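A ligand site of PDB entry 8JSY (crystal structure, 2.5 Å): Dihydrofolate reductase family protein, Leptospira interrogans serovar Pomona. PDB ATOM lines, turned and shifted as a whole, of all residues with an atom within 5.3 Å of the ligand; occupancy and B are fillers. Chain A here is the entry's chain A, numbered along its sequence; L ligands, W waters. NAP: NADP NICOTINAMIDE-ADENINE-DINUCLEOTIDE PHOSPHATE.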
ATOM      1  N   LEU A   7     -10.325  -0.578  17.845  1.00  0.00           N
ATOM      2  CA  LEU A   7      -9.160  -0.280  17.023  1.00  0.00           C
ATOM      3  C   LEU A   7      -8.019   0.152  17.935  1.00  0.00           C
ATOM      4  O   LEU A   7      -8.200   1.032  18.769  1.00  0.00           O
ATOM      5  CB  LEU A   7      -9.477   0.794  15.990  1.00  0.00           C
ATOM      6  CG  LEU A   7     -10.528   0.399  14.959  1.00  0.00           C
ATOM      7  CD1 LEU A   7     -11.907   0.844  15.381  1.00  0.00           C
ATOM      8  CD2 LEU A   7     -10.153   0.973  13.596  1.00  0.00           C
ATOM      9  N   SER A   8      -6.853  -0.472  17.779  1.00  0.00           N
ATOM     10  CA  SER A   8      -5.804  -0.214  18.759  1.00  0.00           C
ATOM     11  C   SER A   8      -4.413  -0.306  18.134  1.00  0.00           C
ATOM     12  O   SER A   8      -4.161  -1.167  17.275  1.00  0.00           O
ATOM     13  CB  SER A   8      -5.912  -1.187  19.936  1.00  0.00           C
ATOM     14  OG  SER A   8      -5.660  -0.565  21.183  1.00  0.00           O
ATOM     15  N   PHE A   9      -3.532   0.573  18.581  1.00  0.00           N
ATOM     16  CA  PHE A   9      -2.099   0.483  18.312  1.00  0.00           C
ATOM     17  C   PHE A   9      -1.458  -0.182  19.516  1.00  0.00           C
ATOM     18  O   PHE A   9      -1.706   0.240  20.654  1.00  0.00           O
ATOM     19  CB  PHE A   9      -1.460   1.865  18.098  1.00  0.00           C
ATOM     20  CG  PHE A   9      -2.027   2.661  16.954  1.00  0.00           C
ATOM     21  CD1 PHE A   9      -3.033   2.164  16.146  1.00  0.00           C
ATOM     22  CD2 PHE A   9      -1.545   3.943  16.689  1.00  0.00           C
ATOM     23  CE1 PHE A   9      -3.554   2.925  15.107  1.00  0.00           C
ATOM     24  CE2 PHE A   9      -2.054   4.695  15.642  1.00  0.00           C
ATOM     25  CZ  PHE A   9      -3.059   4.181  14.857  1.00  0.00           C
ATOM     26  N   ILE A  10      -0.653  -1.220  19.304  1.00  0.00           N
ATOM     27  CA  ILE A  10      -0.013  -1.879  20.433  1.00  0.00           C
ATOM     28  C   ILE A  10       1.434  -2.231  20.105  1.00  0.00           C
ATOM     29  O   ILE A  10       1.819  -2.446  18.949  1.00  0.00           O
ATOM     30  CB  ILE A  10      -0.760  -3.149  20.926  1.00  0.00           C
ATOM     31  CG1 ILE A  10      -0.924  -4.172  19.805  1.00  0.00           C
ATOM     32  CG2 ILE A  10      -2.134  -2.795  21.518  1.00  0.00           C
ATOM     33  CD1 ILE A  10      -1.729  -5.353  20.227  1.00  0.00           C
ATOM     34  N   MET A  16      -0.311   0.113  25.028  1.00  0.00           N
ATOM     35  CA  MET A  16      -1.008   1.035  24.148  1.00  0.00           C
ATOM     36  C   MET A  16      -1.031   2.481  24.650  1.00  0.00           C
ATOM     37  O   MET A  16      -1.600   3.357  23.986  1.00  0.00           O
ATOM     38  CB  MET A  16      -2.441   0.538  23.906  1.00  0.00           C
ATOM     39  CG  MET A  16      -3.146   0.093  25.171  1.00  0.00           C
ATOM     40  SD  MET A  16      -4.419   1.280  25.727  1.00  0.00           S
ATOM     41  CE  MET A  16      -5.720   1.067  24.510  1.00  0.00           C
ATOM     42  N   GLN A  17      -0.411   2.759  25.800  1.00  0.00           N
ATOM     43  CA  GLN A  17      -0.422   4.112  26.355  1.00  0.00           C
ATOM     44  C   GLN A  17       0.370   5.071  25.478  1.00  0.00           C
ATOM     45  O   GLN A  17       1.534   4.829  25.152  1.00  0.00           O
ATOM     46  CB  GLN A  17       0.175   4.097  27.764  1.00  0.00           C
ATOM     47  CG  GLN A  17       0.362   5.463  28.407  1.00  0.00           C
ATOM     48  CD  GLN A  17       0.706   5.316  29.881  1.00  0.00           C
ATOM     49  OE1 GLN A  17       0.630   4.212  30.439  1.00  0.00           O
ATOM     50  NE2 GLN A  17       1.070   6.414  30.523  1.00  0.00           N
ATOM     51  N   ALA A  18      -0.275   6.182  25.106  1.00  0.00           N
ATOM     52  CA  ALA A  18       0.376   7.326  24.485  1.00  0.00           C
ATOM     53  C   ALA A  18       1.096   6.983  23.170  1.00  0.00           C
ATOM     54  O   ALA A  18       2.313   7.203  23.042  1.00  0.00           O
ATOM     55  CB  ALA A  18       1.357   7.950  25.481  1.00  0.00           C
ATOM     56  N   PRO A  19       0.387   6.455  22.170  1.00  0.00           N
ATOM     57  CA  PRO A  19       1.040   6.220  20.878  1.00  0.00           C
ATOM     58  C   PRO A  19       1.544   7.480  20.203  1.00  0.00           C
ATOM     59  O   PRO A  19       2.669   7.490  19.670  1.00  0.00           O
ATOM     60  CB  PRO A  19      -0.068   5.561  20.041  1.00  0.00           C
ATOM     61  CG  PRO A  19      -1.325   6.033  20.636  1.00  0.00           C
ATOM     62  CD  PRO A  19      -1.046   6.112  22.126  1.00  0.00           C
ATOM     63  N   GLU A  24       1.074  12.636  25.453  1.00  0.00           N
ATOM     64  CA  GLU A  24      -0.322  12.150  25.271  1.00  0.00           C
ATOM     65  C   GLU A  24      -0.829  11.544  26.572  1.00  0.00           C
ATOM     66  O   GLU A  24      -1.986  11.808  26.933  1.00  0.00           O
ATOM     67  CB  GLU A  24      -0.408  11.167  24.114  1.00  0.00           C
ATOM     68  CG  GLU A  24      -1.830  10.737  23.797  1.00  0.00           C
ATOM     69  CD  GLU A  24      -1.901   9.719  22.666  1.00  0.00           C
ATOM     70  OE1 GLU A  24      -1.048   9.791  21.777  1.00  0.00           O
ATOM     71  OE2 GLU A  24      -2.803   8.881  22.688  1.00  0.00           O
ATOM     72  N   ASP A  25      -0.005  10.759  27.274  1.00  0.00           N
ATOM     73  CA  ASP A  25      -0.392  10.191  28.597  1.00  0.00           C
ATOM     74  C   ASP A  25       0.859  10.047  29.445  1.00  0.00           C
ATOM     75  O   ASP A  25       1.689   9.185  29.144  1.00  0.00           O
ATOM     76  CB  ASP A  25      -1.143   8.866  28.478  1.00  0.00           C
ATOM     77  CG  ASP A  25      -1.780   8.410  29.776  1.00  0.00           C
ATOM     78  OD1 ASP A  25      -1.698   9.156  30.761  1.00  0.00           O
ATOM     79  OD2 ASP A  25      -2.356   7.320  29.774  1.00  0.00           O
ATOM     80  N   TRP A  35       5.811   6.490  20.690  1.00  0.00           N
ATOM     81  CA  TRP A  35       6.493   5.308  20.143  1.00  0.00           C
ATOM     82  C   TRP A  35       5.937   4.892  18.776  1.00  0.00           C
ATOM     83  O   TRP A  35       6.629   4.187  18.031  1.00  0.00           O
ATOM     84  CB  TRP A  35       6.433   4.140  21.132  1.00  0.00           C
ATOM     85  CG  TRP A  35       5.058   3.846  21.613  1.00  0.00           C
ATOM     86  CD1 TRP A  35       4.451   4.377  22.719  1.00  0.00           C
ATOM     87  CD2 TRP A  35       4.087   2.988  20.990  1.00  0.00           C
ATOM     88  NE1 TRP A  35       3.166   3.894  22.827  1.00  0.00           N
ATOM     89  CE2 TRP A  35       2.912   3.041  21.787  1.00  0.00           C
ATOM     90  CE3 TRP A  35       4.089   2.169  19.864  1.00  0.00           C
ATOM     91  CZ2 TRP A  35       1.773   2.303  21.479  1.00  0.00           C
ATOM     92  CZ3 TRP A  35       2.958   1.443  19.556  1.00  0.00           C
ATOM     93  CH2 TRP A  35       1.807   1.514  20.356  1.00  0.00           C
ATOM     94  N   GLY A  60     -13.841   6.202  26.415  1.00  0.00           N
ATOM     95  CA  GLY A  60     -13.627   6.606  27.791  1.00  0.00           C
ATOM     96  C   GLY A  60     -13.394   8.100  27.887  1.00  0.00           C
ATOM     97  O   GLY A  60     -12.907   8.742  26.945  1.00  0.00           O
ATOM     98  N   ARG A  61     -13.770   8.697  29.023  1.00  0.00           N
ATOM     99  CA  ARG A  61     -13.735  10.155  29.094  1.00  0.00           C
ATOM    100  C   ARG A  61     -12.344  10.685  28.767  1.00  0.00           C
ATOM    101  O   ARG A  61     -12.210  11.711  28.083  1.00  0.00           O
ATOM    102  CB  ARG A  61     -14.163  10.667  30.471  1.00  0.00           C
ATOM    103  CG  ARG A  61     -13.384  11.948  30.794  1.00  0.00           C
ATOM    104  CD  ARG A  61     -13.700  12.543  32.086  1.00  0.00           C
ATOM    105  NE  ARG A  61     -13.022  11.918  33.212  1.00  0.00           N
ATOM    106  CZ  ARG A  61     -11.742  12.094  33.529  1.00  0.00           C
ATOM    107  NH1 ARG A  61     -10.896  12.681  32.712  1.00  0.00           N
ATOM    108  NH2 ARG A  61     -11.300  11.644  34.711  1.00  0.00           N
ATOM    109  N   LYS A  62     -11.294  10.003  29.250  1.00  0.00           N
ATOM    110  CA  LYS A  62      -9.950  10.509  29.032  1.00  0.00           C
ATOM    111  C   LYS A  62      -9.617  10.566  27.543  1.00  0.00           C
ATOM    112  O   LYS A  62      -9.111  11.583  27.056  1.00  0.00           O
ATOM    113  CB  LYS A  62      -8.938   9.674  29.792  1.00  0.00           C
ATOM    114  CG  LYS A  62      -8.986   9.945  31.285  1.00  0.00           C
ATOM    115  CD  LYS A  62      -8.347   8.818  32.047  1.00  0.00           C
ATOM    116  CE  LYS A  62      -8.297   9.098  33.523  1.00  0.00           C
ATOM    117  NZ  LYS A  62      -7.855   7.863  34.204  1.00  0.00           N
ATOM    118  N   THR A  63      -9.931   9.500  26.816  1.00  0.00           N
ATOM    119  CA  THR A  63      -9.698   9.498  25.376  1.00  0.00           C
ATOM    120  C   THR A  63     -10.589  10.509  24.673  1.00  0.00           C
ATOM    121  O   THR A  63     -10.162  11.158  23.703  1.00  0.00           O
ATOM    122  CB  THR A  63      -9.908   8.090  24.809  1.00  0.00           C
ATOM    123  OG1 THR A  63      -8.883   7.237  25.324  1.00  0.00           O
ATOM    124  CG2 THR A  63      -9.842   8.081  23.284  1.00  0.00           C
ATOM    125  N   PHE A  64     -11.835  10.668  25.145  1.00  0.00           N
ATOM    126  CA  PHE A  64     -12.706  11.678  24.556  1.00  0.00           C
ATOM    127  C   PHE A  64     -12.091  13.064  24.693  1.00  0.00           C
ATOM    128  O   PHE A  64     -12.120  13.857  23.750  1.00  0.00           O
ATOM    129  CB  PHE A  64     -14.081  11.674  25.204  1.00  0.00           C
ATOM    130  CG  PHE A  64     -14.951  12.819  24.772  1.00  0.00           C
ATOM    131  CD1 PHE A  64     -15.417  12.902  23.461  1.00  0.00           C
ATOM    132  CD2 PHE A  64     -15.287  13.842  25.652  1.00  0.00           C
ATOM    133  CE1 PHE A  64     -16.213  13.971  23.046  1.00  0.00           C
ATOM    134  CE2 PHE A  64     -16.088  14.923  25.238  1.00  0.00           C
ATOM    135  CZ  PHE A  64     -16.549  14.977  23.932  1.00  0.00           C
ATOM    136  N   ILE A  66      -8.817  13.899  25.230  1.00  0.00           N
ATOM    137  CA  ILE A  66      -7.675  13.968  24.314  1.00  0.00           C
ATOM    138  C   ILE A  66      -8.136  14.276  22.889  1.00  0.00           C
ATOM    139  O   ILE A  66      -7.584  15.158  22.217  1.00  0.00           O
ATOM    140  CB  ILE A  66      -6.891  12.653  24.372  1.00  0.00           C
ATOM    141  CG1 ILE A  66      -6.558  12.298  25.838  1.00  0.00           C
ATOM    142  CG2 ILE A  66      -5.744  12.655  23.359  1.00  0.00           C
ATOM    143  CD1 ILE A  66      -5.638  11.074  26.012  1.00  0.00           C
ATOM    144  N   PHE A  67      -9.164  13.567  22.401  1.00  0.00           N
ATOM    145  CA  PHE A  67      -9.663  13.842  21.044  1.00  0.00           C
ATOM    146  C   PHE A  67     -10.261  15.250  20.922  1.00  0.00           C
ATOM    147  O   PHE A  67     -10.010  15.951  19.939  1.00  0.00           O
ATOM    148  CB  PHE A  67     -10.703  12.775  20.647  1.00  0.00           C
ATOM    149  CG  PHE A  67     -10.089  11.518  20.064  1.00  0.00           C
ATOM    150  CD1 PHE A  67      -8.710  11.361  19.996  1.00  0.00           C
ATOM    151  CD2 PHE A  67     -10.897  10.494  19.608  1.00  0.00           C
ATOM    152  CE1 PHE A  67      -8.144  10.209  19.468  1.00  0.00           C
ATOM    153  CE2 PHE A  67     -10.346   9.336  19.076  1.00  0.00           C
ATOM    154  CZ  PHE A  67      -8.967   9.195  19.003  1.00  0.00           C
ATOM    155  N   MET A  89     -18.287   7.396  28.008  1.00  0.00           N
ATOM    156  CA  MET A  89     -18.558   6.851  29.325  1.00  0.00           C
ATOM    157  C   MET A  89     -17.941   7.772  30.362  1.00  0.00           C
ATOM    158  O   MET A  89     -16.722   7.953  30.401  1.00  0.00           O
ATOM    159  CB  MET A  89     -17.990   5.430  29.438  1.00  0.00           C
ATOM    160  CG  MET A  89     -18.294   4.753  30.753  1.00  0.00           C
ATOM    161  SD  MET A  89     -19.853   3.843  30.701  1.00  0.00           S
ATOM    162  CE  MET A  89     -19.850   3.129  32.347  1.00  0.00           C
ATOM    163  N   SER A  90     -18.780   8.384  31.196  1.00  0.00           N
ATOM    164  CA  SER A  90     -18.212   9.244  32.224  1.00  0.00           C
ATOM    165  C   SER A  90     -19.237   9.487  33.320  1.00  0.00           C
ATOM    166  O   SER A  90     -20.446   9.583  33.046  1.00  0.00           O
ATOM    167  CB  SER A  90     -17.749  10.587  31.632  1.00  0.00           C
ATOM    168  OG  SER A  90     -17.303  11.470  32.640  1.00  0.00           O
ATOM    169  N   LYS A  91     -18.744   9.572  34.553  1.00  0.00           N
ATOM    170  CA  LYS A  91     -19.539  10.062  35.673  1.00  0.00           C
ATOM    171  C   LYS A  91     -19.269  11.530  35.979  1.00  0.00           C
ATOM    172  O   LYS A  91     -20.105  12.160  36.639  1.00  0.00           O
ATOM    173  CB  LYS A  91     -19.261   9.238  36.935  1.00  0.00           C
ATOM    174  CG  LYS A  91     -19.458   7.759  36.776  1.00  0.00           C
ATOM    175  CD  LYS A  91     -20.937   7.409  36.836  1.00  0.00           C
ATOM    176  CE  LYS A  91     -21.155   5.895  36.946  1.00  0.00           C
ATOM    177  NZ  LYS A  91     -22.572   5.505  36.642  1.00  0.00           N
ATOM    178  N   THR A  92     -18.149  12.088  35.509  1.00  0.00           N
ATOM    179  CA  THR A  92     -17.774  13.451  35.864  1.00  0.00           C
ATOM    180  C   THR A  92     -18.046  14.466  34.766  1.00  0.00           C
ATOM    181  O   THR A  92     -17.878  15.667  34.998  1.00  0.00           O
ATOM    182  CB  THR A  92     -16.290  13.530  36.230  1.00  0.00           C
ATOM    183  OG1 THR A  92     -15.505  13.107  35.107  1.00  0.00           O
ATOM    184  CG2 THR A  92     -15.969  12.684  37.445  1.00  0.00           C
ATOM    185  N   VAL A  93     -18.406  14.033  33.563  1.00  0.00           N
ATOM    186  CA  VAL A  93     -18.724  14.969  32.496  1.00  0.00           C
ATOM    187  C   VAL A  93     -20.103  14.648  31.975  1.00  0.00           C
ATOM    188  O   VAL A  93     -20.450  13.470  31.787  1.00  0.00           O
ATOM    189  CB  VAL A  93     -17.679  14.942  31.360  1.00  0.00           C
ATOM    190  CG1 VAL A  93     -18.061  15.941  30.308  1.00  0.00           C
ATOM    191  CG2 VAL A  93     -16.291  15.258  31.902  1.00  0.00           C
ATOM    192  N   GLU A 105     -23.445   6.541  31.501  1.00  0.00           N
ATOM    193  CA  GLU A 105     -22.883   6.306  32.824  1.00  0.00           C
ATOM    194  C   GLU A 105     -22.768   4.848  33.254  1.00  0.00           C
ATOM    195  O   GLU A 105     -22.076   4.579  34.241  1.00  0.00           O
ATOM    196  CB  GLU A 105     -23.699   7.057  33.887  1.00  0.00           C
ATOM    197  CG  GLU A 105     -23.484   8.549  33.823  1.00  0.00           C
ATOM    198  CD  GLU A 105     -24.439   9.322  34.705  1.00  0.00           C
ATOM    199  OE1 GLU A 105     -24.582   8.950  35.899  1.00  0.00           O
ATOM    200  OE2 GLU A 105     -25.038  10.294  34.206  1.00  0.00           O
ATOM    201  N   TRP A 124     -11.831   3.826  20.037  1.00  0.00           N
ATOM    202  CA  TRP A 124     -10.439   4.216  19.879  1.00  0.00           C
ATOM    203  C   TRP A 124      -9.882   4.537  21.253  1.00  0.00           C
ATOM    204  O   TRP A 124     -10.624   4.956  22.138  1.00  0.00           O
ATOM    205  CB  TRP A 124     -10.279   5.431  18.973  1.00  0.00           C
ATOM    206  CG  TRP A 124     -10.777   5.232  17.590  1.00  0.00           C
ATOM    207  CD1 TRP A 124     -12.080   5.266  17.168  1.00  0.00           C
ATOM    208  CD2 TRP A 124      -9.990   4.961  16.433  1.00  0.00           C
ATOM    209  NE1 TRP A 124     -12.147   5.045  15.818  1.00  0.00           N
ATOM    210  CE2 TRP A 124     -10.875   4.852  15.336  1.00  0.00           C
ATOM    211  CE3 TRP A 124      -8.622   4.814  16.204  1.00  0.00           C
ATOM    212  CZ2 TRP A 124     -10.432   4.591  14.044  1.00  0.00           C
ATOM    213  CZ3 TRP A 124      -8.176   4.551  14.928  1.00  0.00           C
ATOM    214  CH2 TRP A 124      -9.079   4.447  13.863  1.00  0.00           C
ATOM    215  N   GLY A 125      -8.571   4.350  21.424  1.00  0.00           N
ATOM    216  CA  GLY A 125      -7.996   4.528  22.751  1.00  0.00           C
ATOM    217  C   GLY A 125      -8.817   3.776  23.778  1.00  0.00           C
ATOM    218  O   GLY A 125      -9.179   2.608  23.581  1.00  0.00           O
ATOM    219  N   SER A 126      -9.133   4.459  24.887  1.00  0.00           N
ATOM    220  CA  SER A 126     -10.136   4.012  25.854  1.00  0.00           C
ATOM    221  C   SER A 126      -9.774   2.658  26.493  1.00  0.00           C
ATOM    222  O   SER A 126     -10.561   1.706  26.474  1.00  0.00           O
ATOM    223  CB  SER A 126     -11.516   3.953  25.205  1.00  0.00           C
ATOM    224  OG  SER A 126     -11.732   5.023  24.306  1.00  0.00           O
ATOM    225  N   GLY A 127      -8.582   2.604  27.084  1.00  0.00           N
ATOM    226  CA  GLY A 127      -8.095   1.341  27.625  1.00  0.00           C
ATOM    227  C   GLY A 127      -8.956   0.819  28.759  1.00  0.00           C
ATOM    228  O   GLY A 127      -9.313  -0.360  28.793  1.00  0.00           O
ATOM    229  N   GLU A 128      -9.304   1.698  29.699  1.00  0.00           N
ATOM    230  CA  GLU A 128     -10.148   1.302  30.831  1.00  0.00           C
ATOM    231  C   GLU A 128     -11.543   0.890  30.366  1.00  0.00           C
ATOM    232  O   GLU A 128     -12.069  -0.175  30.773  1.00  0.00           O
ATOM    233  CB  GLU A 128     -10.225   2.477  31.804  1.00  0.00           C
ATOM    234  CG  GLU A 128     -10.952   2.186  33.072  1.00  0.00           C
ATOM    235  CD  GLU A 128     -10.708   3.253  34.116  1.00  0.00           C
ATOM    236  OE1 GLU A 128     -10.169   4.337  33.749  1.00  0.00           O
ATOM    237  OE2 GLU A 128     -11.036   3.000  35.294  1.00  0.00           O
ATOM    238  N   LEU A 129     -12.152   1.710  29.519  1.00  0.00           N
ATOM    239  CA  LEU A 129     -13.456   1.362  28.983  1.00  0.00           C
ATOM    240  C   LEU A 129     -13.377   0.032  28.265  1.00  0.00           C
ATOM    241  O   LEU A 129     -14.282  -0.808  28.391  1.00  0.00           O
ATOM    242  CB  LEU A 129     -13.963   2.442  28.036  1.00  0.00           C
ATOM    243  CG  LEU A 129     -15.411   2.156  27.635  1.00  0.00           C
ATOM    244  CD1 LEU A 129     -16.272   2.000  28.889  1.00  0.00           C
ATOM    245  CD2 LEU A 129     -15.981   3.204  26.712  1.00  0.00           C
ATOM    246  N   ILE A 130     -12.297  -0.194  27.518  1.00  0.00           N
ATOM    247  CA  ILE A 130     -12.126  -1.450  26.798  1.00  0.00           C
ATOM    248  C   ILE A 130     -12.095  -2.621  27.772  1.00  0.00           C
ATOM    249  O   ILE A 130     -12.593  -3.717  27.459  1.00  0.00           O
ATOM    250  CB  ILE A 130     -10.856  -1.397  25.943  1.00  0.00           C
ATOM    251  CG1 ILE A 130     -11.160  -0.713  24.620  1.00  0.00           C
ATOM    252  CG2 ILE A 130     -10.280  -2.802  25.747  1.00  0.00           C
ATOM    253  CD1 ILE A 130      -9.917  -0.504  23.797  1.00  0.00           C
ATOM    254  N   LEU A 132     -13.812  -2.809  30.481  1.00  0.00           N
ATOM    255  CA  LEU A 132     -15.240  -3.067  30.724  1.00  0.00           C
ATOM    256  C   LEU A 132     -15.907  -3.786  29.550  1.00  0.00           C
ATOM    257  O   LEU A 132     -16.736  -4.685  29.752  1.00  0.00           O
ATOM    258  CB  LEU A 132     -15.978  -1.754  31.010  1.00  0.00           C
ATOM    259  CG  LEU A 132     -17.495  -1.911  31.157  1.00  0.00           C
ATOM    260  CD1 LEU A 132     -17.819  -2.478  32.531  1.00  0.00           C
ATOM    261  CD2 LEU A 132     -18.225  -0.588  30.942  1.00  0.00           C
ATOM    262  N   LYS A 155      -0.055   1.417  30.022  1.00  0.00           N
ATOM    263  CA  LYS A 155      -1.373   0.822  29.983  1.00  0.00           C
ATOM    264  C   LYS A 155      -1.452  -0.216  28.864  1.00  0.00           C
ATOM    265  O   LYS A 155      -0.813  -0.087  27.814  1.00  0.00           O
ATOM    266  CB  LYS A 155      -2.437   1.906  29.826  1.00  0.00           C
ATOM    267  CG  LYS A 155      -2.602   2.773  31.059  1.00  0.00           C
ATOM    268  CD  LYS A 155      -3.140   4.165  30.726  1.00  0.00           C
ATOM    269  CE  LYS A 155      -3.324   5.029  31.985  1.00  0.00           C
ATOM    270  NZ  LYS A 155      -4.006   6.325  31.711  1.00  0.00           N
HETATM  271  PA  NAP L   1     -10.203   6.049  29.082  1.00  0.00           P
HETATM  272  O1A NAP L   1     -10.738   4.657  28.901  1.00  0.00           O
HETATM  273  O2A NAP L   1      -9.970   6.696  27.738  1.00  0.00           O
HETATM  274  O5B NAP L   1     -11.262   6.920  29.991  1.00  0.00           O
HETATM  275  C5B NAP L   1     -11.226   6.630  31.371  1.00  0.00           C
HETATM  276  C4B NAP L   1     -12.508   7.264  31.941  1.00  0.00           C
HETATM  277  O4B NAP L   1     -13.535   6.830  31.272  1.00  0.00           O
HETATM  278  C3B NAP L   1     -12.761   6.849  33.384  1.00  0.00           C
HETATM  279  O3B NAP L   1     -12.101   7.689  34.232  1.00  0.00           O
HETATM  280  C2B NAP L   1     -14.308   6.984  33.435  1.00  0.00           C
HETATM  281  O2B NAP L   1     -14.747   8.421  33.372  1.00  0.00           O
HETATM  282  C1B NAP L   1     -14.686   6.402  32.315  1.00  0.00           C
HETATM  283  N9A NAP L   1     -14.703   4.962  32.382  1.00  0.00           N
HETATM  284  C8A NAP L   1     -13.932   4.093  31.703  1.00  0.00           C
HETATM  285  N7A NAP L   1     -14.251   2.847  32.050  1.00  0.00           N
HETATM  286  C5A NAP L   1     -15.247   2.926  32.956  1.00  0.00           C
HETATM  287  C6A NAP L   1     -15.949   1.949  33.635  1.00  0.00           C
HETATM  288  N6A NAP L   1     -15.632   0.568  33.400  1.00  0.00           N
HETATM  289  N1A NAP L   1     -16.901   2.288  34.488  1.00  0.00           N
HETATM  290  C2A NAP L   1     -17.197   3.586  34.712  1.00  0.00           C
HETATM  291  N3A NAP L   1     -16.510   4.547  34.039  1.00  0.00           N
HETATM  292  C4A NAP L   1     -15.531   4.223  33.161  1.00  0.00           C
HETATM  293  O3  NAP L   1      -8.887   6.087  30.058  1.00  0.00           O
HETATM  294  PN  NAP L   1      -7.370   5.599  29.694  1.00  0.00           P
HETATM  295  O1N NAP L   1      -7.499   4.284  28.953  1.00  0.00           O
HETATM  296  O2N NAP L   1      -6.581   5.481  30.979  1.00  0.00           O
HETATM  297  O5D NAP L   1      -6.684   6.722  28.708  1.00  0.00           O
HETATM  298  C5D NAP L   1      -6.763   6.466  27.340  1.00  0.00           C
HETATM  299  C4D NAP L   1      -5.407   5.863  26.897  1.00  0.00           C
HETATM  300  O4D NAP L   1      -5.545   5.473  25.670  1.00  0.00           O
HETATM  301  C3D NAP L   1      -4.285   6.936  26.883  1.00  0.00           C
HETATM  302  O3D NAP L   1      -3.129   6.404  27.377  1.00  0.00           O
HETATM  303  C2D NAP L   1      -4.130   7.279  25.390  1.00  0.00           C
HETATM  304  O2D NAP L   1      -2.749   7.803  25.157  1.00  0.00           O
HETATM  305  C1D NAP L   1      -4.287   6.086  24.878  1.00  0.00           C
HETATM  306  N1N NAP L   1      -4.653   6.003  23.497  1.00  0.00           N
HETATM  307  C2N NAP L   1      -4.279   4.909  22.819  1.00  0.00           C
HETATM  308  C3N NAP L   1      -4.630   4.757  21.492  1.00  0.00           C
HETATM  309  C7N NAP L   1      -4.159   3.500  20.773  1.00  0.00           C
HETATM  310  O7N NAP L   1      -4.786   3.048  19.872  1.00  0.00           O
HETATM  311  N7N NAP L   1      -2.938   2.853  21.239  1.00  0.00           N
HETATM  312  C4N NAP L   1      -5.355   5.707  20.849  1.00  0.00           C
HETATM  313  C5N NAP L   1      -5.736   6.806  21.523  1.00  0.00           C
HETATM  314  C6N NAP L   1      -5.391   6.945  22.867  1.00  0.00           C
HETATM  315  P2B NAP L   1     -14.979   9.423  34.676  1.00  0.00           P
HETATM  316  O1X NAP L   1     -15.292  10.779  34.090  1.00  0.00           O
HETATM  317  O2X NAP L   1     -16.144   8.989  35.528  1.00  0.00           O
HETATM  318  O3X NAP L   1     -13.750   9.595  35.545  1.00  0.00           O
HETATM  319  O   HOH W   1      -7.486   3.446  19.214  1.00  0.00           O
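The backbone NH of Leu 129 is in hydrogen-bond range of an oxygen (O1A) of the ligand (3.3 Å).
OG of Ser 90 sits at hydrogen-bond distance from O1X of the ligand (2.6 Å).
The backbone NH of Thr 92 is in hydrogen-bond range of an oxygen (O1X) of the ligand, at 3.4 Å.
The backbone NH of Lys 62 sits at hydrogen-bond distance from an oxygen (O5B) of the ligand (3.2 Å).
An oxygen (O1X) of the ligand lies within salt-bridge range of the guanidinium group of Arg 61 (2.7 Å).
N of Arg 61 lies within hydrogen-bond range of O4B of the ligand (2.9 Å).
The backbone NH (N) of Thr 63 is in hydrogen-bond range of an oxygen (O2A) of the ligand (3.0 Å).
An oxygen (O1X) of the ligand lies within hydrogen-bond range of the side-chain hydroxyl (OG1) of Thr 92 (2.5 Å).
The backbone NH (N) of Lys 91 sits at hydrogen-bond distance from an oxygen (O2X) of the ligand (2.8 Å).
O of Phe 9 is in hydrogen-bond range of N7N of the ligand, at 2.9 Å.
N of Ala 18 sits at hydrogen-bond distance from O2D of the ligand (3.0 Å).
NZ of Lys 155 is in salt-bridge range of O2N of the ligand (2.8 Å).
An oxygen (O1N) of the ligand sits at hydrogen-bond distance from the backbone NH (N) of Gly 127 (2.7 Å).
OG1 of Thr 63 is in hydrogen-bond range of O2A of the ligand (2.7 Å).
N of Phe 9 lies within hydrogen-bond range of O7N of the ligand, at 3.1 Å.
N7N of the ligand lies within hydrogen-bond range of O of Met 16, 3.1 Å away.
The side-chain carboxylate (OD2) of Asp 25 lies within hydrogen-bond range of an oxygen (O3D) of the ligand.
OE2 of Glu 24 sits at hydrogen-bond distance from O2D of the ligand.
N of Glu 128 lies within hydrogen-bond range of O1N of the ligand, 3.2 Å away.
The backbone NH (N) of Val 93 is in hydrogen-bond range of the side-chain hydroxyl (OG) of Ser 90 (2.9 Å).
The backbone carbonyl oxygen of Glu 105 sits at hydrogen-bond distance from the side-chain amino group of Lys 91 (2.6 Å).
O of Lys 155 lies within hydrogen-bond range of N of Met 16 (2.8 Å).
O of Ala 18 lies within hydrogen-bond range of NE1 of Trp 35, at 3.4 Å.
N of Trp 35 is in hydrogen-bond range of O of Pro 19 (3.5 Å).
N of Ser 126 is in hydrogen-bond range of OG1 of Thr 63 (2.8 Å).
The side-chain hydroxyl (OG) of Ser 126 is in hydrogen-bond range of the backbone carbonyl oxygen (O) of Trp 124 (2.4 Å).
The side-chain carboxylate of Asp 25 is in salt-bridge range of the side-chain amino group of Lys 155 (2.7 Å).
An oxygen (O4B) of the ligand lies close to the backbone carbonyl oxygen (O) of Met 89, at 3.5 Å.
Residues that only touch the ligand: Ser 126 (3.2 Å), Gly 60 (3.2 Å), Leu 132 (3.4 Å), Gly 125 (3.4 Å), Pro 19 (3.5 Å), Ser 8 (3.6 Å) and Gln 17 (3.7 Å).
Hydrophobic or aromatic side chains that line the ligand: Phe 9, Met 16, Pro 19, Met 89, Leu 129 and Leu 132.
Of the 33 residues printed, 23 come within 4 Å of the ligand.
The nearest printed residue that does not touch the ligand is Leu 7 (4.1 Å).
Water W1 lies within hydrogen-bond range of the backbone carbonyl oxygen (O) of Leu 7 (2.6 Å), the backbone NH (N) of Gly 125 (2.6 Å) and an oxygen (O7N) of the ligand (2.8 Å).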
